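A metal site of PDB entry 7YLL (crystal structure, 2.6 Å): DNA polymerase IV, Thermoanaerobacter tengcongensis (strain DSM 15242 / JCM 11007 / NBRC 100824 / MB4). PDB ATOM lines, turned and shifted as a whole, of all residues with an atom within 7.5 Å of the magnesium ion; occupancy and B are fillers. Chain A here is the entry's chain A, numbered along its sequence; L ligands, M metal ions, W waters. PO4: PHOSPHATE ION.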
ATOM      1  N   VAL A   8      20.430  15.155   2.795  1.00  0.00           N
ATOM      2  CA  VAL A   8      19.535  15.094   1.660  1.00  0.00           C
ATOM      3  C   VAL A   8      19.262  16.513   1.155  1.00  0.00           C
ATOM      4  O   VAL A   8      19.203  17.450   1.923  1.00  0.00           O
ATOM      5  CB  VAL A   8      18.226  14.360   1.961  1.00  0.00           C
ATOM      6  CG1 VAL A   8      18.484  12.875   2.126  1.00  0.00           C
ATOM      7  CG2 VAL A   8      17.569  14.921   3.201  1.00  0.00           C
ATOM      8  N   ASP A   9      19.115  16.650  -0.154  1.00  0.00           N
ATOM      9  CA  ASP A   9      18.937  17.959  -0.744  1.00  0.00           C
ATOM     10  C   ASP A   9      18.240  17.754  -2.081  1.00  0.00           C
ATOM     11  O   ASP A   9      18.828  17.193  -3.015  1.00  0.00           O
ATOM     12  CB  ASP A   9      20.285  18.664  -0.908  1.00  0.00           C
ATOM     13  CG  ASP A   9      20.137  20.094  -1.351  1.00  0.00           C
ATOM     14  OD1 ASP A   9      19.103  20.447  -1.958  1.00  0.00           O
ATOM     15  OD2 ASP A   9      21.058  20.894  -1.111  1.00  0.00           O
ATOM     16  N   MET A  10      16.994  18.204  -2.166  1.00  0.00           N
ATOM     17  CA  MET A  10      16.214  18.071  -3.388  1.00  0.00           C
ATOM     18  C   MET A  10      16.811  18.928  -4.493  1.00  0.00           C
ATOM     19  O   MET A  10      17.323  20.029  -4.253  1.00  0.00           O
ATOM     20  CB  MET A  10      14.772  18.487  -3.122  1.00  0.00           C
ATOM     21  CG  MET A  10      14.124  17.674  -2.015  1.00  0.00           C
ATOM     22  SD  MET A  10      13.787  15.956  -2.484  1.00  0.00           S
ATOM     23  CE  MET A  10      12.825  16.076  -3.980  1.00  0.00           C
ATOM     24  N   ASP A  11      16.773  18.390  -5.719  1.00  0.00           N
ATOM     25  CA  ASP A  11      17.340  19.054  -6.901  1.00  0.00           C
ATOM     26  C   ASP A  11      16.343  20.073  -7.449  1.00  0.00           C
ATOM     27  O   ASP A  11      15.214  19.704  -7.794  1.00  0.00           O
ATOM     28  CB  ASP A  11      17.673  18.059  -8.000  1.00  0.00           C
ATOM     29  CG  ASP A  11      18.624  16.983  -7.550  1.00  0.00           C
ATOM     30  OD1 ASP A  11      19.628  17.303  -6.863  1.00  0.00           O
ATOM     31  OD2 ASP A  11      18.378  15.806  -7.926  1.00  0.00           O
ATOM     32  N   ALA A  12      16.777  21.328  -7.552  1.00  0.00           N
ATOM     33  CA  ALA A  12      15.934  22.393  -8.081  1.00  0.00           C
ATOM     34  C   ALA A  12      14.483  22.150  -7.704  1.00  0.00           C
ATOM     35  O   ALA A  12      13.609  22.096  -8.554  1.00  0.00           O
ATOM     36  CB  ALA A  12      16.091  22.497  -9.583  1.00  0.00           C
ATOM     37  N   PHE A  13      14.256  22.035  -6.396  1.00  0.00           N
ATOM     38  CA  PHE A  13      12.942  21.799  -5.813  1.00  0.00           C
ATOM     39  C   PHE A  13      11.673  22.364  -6.465  1.00  0.00           C
ATOM     40  O   PHE A  13      10.831  21.606  -6.939  1.00  0.00           O
ATOM     41  CB  PHE A  13      12.947  22.253  -4.341  1.00  0.00           C
ATOM     42  CG  PHE A  13      11.935  21.543  -3.490  1.00  0.00           C
ATOM     43  CD1 PHE A  13      11.695  20.195  -3.648  1.00  0.00           C
ATOM     44  CD2 PHE A  13      11.230  22.234  -2.506  1.00  0.00           C
ATOM     45  CE1 PHE A  13      10.771  19.541  -2.860  1.00  0.00           C
ATOM     46  CE2 PHE A  13      10.299  21.584  -1.723  1.00  0.00           C
ATOM     47  CZ  PHE A  13      10.069  20.238  -1.900  1.00  0.00           C
ATOM     48  N   PHE A  14      11.539  23.692  -6.478  1.00  0.00           N
ATOM     49  CA  PHE A  14      10.328  24.297  -7.032  1.00  0.00           C
ATOM     50  C   PHE A  14      10.210  24.036  -8.513  1.00  0.00           C
ATOM     51  O   PHE A  14       9.141  23.713  -9.000  1.00  0.00           O
ATOM     52  CB  PHE A  14      10.272  25.795  -6.743  1.00  0.00           C
ATOM     53  CG  PHE A  14      10.260  26.152  -5.295  1.00  0.00           C
ATOM     54  CD1 PHE A  14      10.071  25.180  -4.332  1.00  0.00           C
ATOM     55  CD2 PHE A  14      10.436  27.449  -4.895  1.00  0.00           C
ATOM     56  CE1 PHE A  14      10.069  25.498  -2.995  1.00  0.00           C
ATOM     57  CE2 PHE A  14      10.433  27.784  -3.562  1.00  0.00           C
ATOM     58  CZ  PHE A  14      10.250  26.808  -2.612  1.00  0.00           C
ATOM     59  N   THR A  43      14.371  29.560  -7.763  1.00  0.00           N
ATOM     60  CA  THR A  43      15.164  28.427  -8.220  1.00  0.00           C
ATOM     61  C   THR A  43      14.906  28.269  -9.708  1.00  0.00           C
ATOM     62  O   THR A  43      13.972  28.866 -10.246  1.00  0.00           O
ATOM     63  CB  THR A  43      14.831  27.154  -7.424  1.00  0.00           C
ATOM     64  OG1 THR A  43      15.930  26.235  -7.510  1.00  0.00           O
ATOM     65  CG2 THR A  43      13.604  26.473  -7.963  1.00  0.00           C
ATOM     66  N   TYR A  46      17.907  22.642 -14.262  1.00  0.00           N
ATOM     67  CA  TYR A  46      19.311  22.529 -14.664  1.00  0.00           C
ATOM     68  C   TYR A  46      19.496  22.917 -16.134  1.00  0.00           C
ATOM     69  O   TYR A  46      20.536  23.501 -16.512  1.00  0.00           O
ATOM     70  CB  TYR A  46      19.820  21.115 -14.325  1.00  0.00           C
ATOM     71  CG  TYR A  46      20.219  21.058 -12.883  1.00  0.00           C
ATOM     72  CD1 TYR A  46      19.266  20.843 -11.879  1.00  0.00           C
ATOM     73  CD2 TYR A  46      21.524  21.313 -12.491  1.00  0.00           C
ATOM     74  CE1 TYR A  46      19.630  20.852 -10.541  1.00  0.00           C
ATOM     75  CE2 TYR A  46      21.895  21.303 -11.162  1.00  0.00           C
ATOM     76  CZ  TYR A  46      20.952  21.082 -10.184  1.00  0.00           C
ATOM     77  OH  TYR A  46      21.315  21.084  -8.853  1.00  0.00           O
ATOM     78  N   ARG A  49      19.897  26.590 -15.732  1.00  0.00           N
ATOM     79  CA  ARG A  49      21.224  26.955 -15.240  1.00  0.00           C
ATOM     80  C   ARG A  49      22.250  26.927 -16.356  1.00  0.00           C
ATOM     81  O   ARG A  49      23.230  27.676 -16.314  1.00  0.00           O
ATOM     82  CB  ARG A  49      21.648  26.032 -14.099  1.00  0.00           C
ATOM     83  CG  ARG A  49      20.873  26.262 -12.839  1.00  0.00           C
ATOM     84  CD  ARG A  49      21.172  25.229 -11.768  1.00  0.00           C
ATOM     85  NE  ARG A  49      20.056  25.096 -10.822  1.00  0.00           N
ATOM     86  CZ  ARG A  49      20.173  24.708  -9.554  1.00  0.00           C
ATOM     87  NH1 ARG A  49      19.106  24.596  -8.779  1.00  0.00           N
ATOM     88  NH2 ARG A  49      21.368  24.395  -9.048  1.00  0.00           N
ATOM     89  N   SER A 101      15.645  22.985   5.750  1.00  0.00           N
ATOM     90  CA  SER A 101      14.810  23.865   4.955  1.00  0.00           C
ATOM     91  C   SER A 101      13.759  23.012   4.299  1.00  0.00           C
ATOM     92  O   SER A 101      13.764  21.788   4.409  1.00  0.00           O
ATOM     93  CB  SER A 101      15.638  24.651   3.932  1.00  0.00           C
ATOM     94  OG  SER A 101      15.937  23.869   2.788  1.00  0.00           O
ATOM     95  N   ASP A 103      13.496  21.901   1.635  1.00  0.00           N
ATOM     96  CA  ASP A 103      14.068  20.833   0.823  1.00  0.00           C
ATOM     97  C   ASP A 103      15.400  20.265   1.299  1.00  0.00           C
ATOM     98  O   ASP A 103      16.080  19.606   0.546  1.00  0.00           O
ATOM     99  CB  ASP A 103      14.187  21.258  -0.649  1.00  0.00           C
ATOM    100  CG  ASP A 103      15.462  22.019  -0.930  1.00  0.00           C
ATOM    101  OD1 ASP A 103      15.854  22.851  -0.105  1.00  0.00           O
ATOM    102  OD2 ASP A 103      16.086  21.793  -1.987  1.00  0.00           O
ATOM    103  N   GLU A 104      15.792  20.509   2.541  1.00  0.00           N
ATOM    104  CA  GLU A 104      17.064  19.975   3.001  1.00  0.00           C
ATOM    105  C   GLU A 104      16.959  19.428   4.412  1.00  0.00           C
ATOM    106  O   GLU A 104      16.440  20.104   5.309  1.00  0.00           O
ATOM    107  CB  GLU A 104      18.178  21.022   2.982  1.00  0.00           C
ATOM    108  CG  GLU A 104      18.724  21.396   1.647  1.00  0.00           C
ATOM    109  CD  GLU A 104      19.798  22.483   1.773  1.00  0.00           C
ATOM    110  OE1 GLU A 104      20.543  22.447   2.780  1.00  0.00           O
ATOM    111  OE2 GLU A 104      19.866  23.377   0.889  1.00  0.00           O
ATOM    112  N   LYS A 154      25.726  17.036  -7.714  1.00  0.00           N
ATOM    113  CA  LYS A 154      24.460  17.750  -7.547  1.00  0.00           C
ATOM    114  C   LYS A 154      23.152  17.275  -8.147  1.00  0.00           C
ATOM    115  O   LYS A 154      22.237  16.948  -7.390  1.00  0.00           O
ATOM    116  CB  LYS A 154      24.658  19.198  -7.985  1.00  0.00           C
ATOM    117  CG  LYS A 154      24.071  20.187  -6.983  1.00  0.00           C
ATOM    118  CD  LYS A 154      22.696  19.734  -6.491  1.00  0.00           C
ATOM    119  CE  LYS A 154      22.497  20.009  -5.011  1.00  0.00           C
ATOM    120  NZ  LYS A 154      21.212  19.433  -4.559  1.00  0.00           N
HETATM  121  P   PO4 L   1      19.639  22.831  -5.862  1.00  0.00           P
HETATM  122  O1  PO4 L   1      21.014  23.465  -6.084  1.00  0.00           O
HETATM  123  O2  PO4 L   1      19.414  21.615  -6.770  1.00  0.00           O
HETATM  124  O3  PO4 L   1      18.543  23.860  -6.156  1.00  0.00           O
HETATM  125  O4  PO4 L   1      19.516  22.425  -4.412  1.00  0.00           O
HETATM  126 MG    MG M   1      17.755  21.933  -3.178  1.00  0.00          MG
HETATM  127  O   HOH W   1      18.293  24.167  -1.902  1.00  0.00           O
HETATM  128  O   HOH W   2      16.412  23.696  -4.696  1.00  0.00           O
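OD1 of Asp 103 is in hydrogen-bond range of OG of Ser 101 (3.1 Å).
The side-chain carboxylate (OD2) of Asp 9 lies within salt-bridge range of the side-chain amino group (NZ) of Lys 154 (3.7 Å).
Of the 14 residues printed, 3 come within 4 Å of the magnesium ion.
The side-chain carboxylate (OD2) of Asp 103 binds the magnesium ion (2.1 Å).
O4 of the ligand is bound to the magnesium ion (2.2 Å).
O of Met 10 is bound to the magnesium ion (2.2 Å).
The side-chain carboxylate (OD1) of Asp 9 binds the magnesium ion, 2.3 Å away.
Slightly farther from the magnesium ion lies water W1 (2.6 Å).
Slightly farther from the magnesium ion lies water W2 (2.7 Å).
Water W1 bridges OE2 of Glu 104 (3.3 Å) and OD1 of Asp 103 (3.3 Å).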
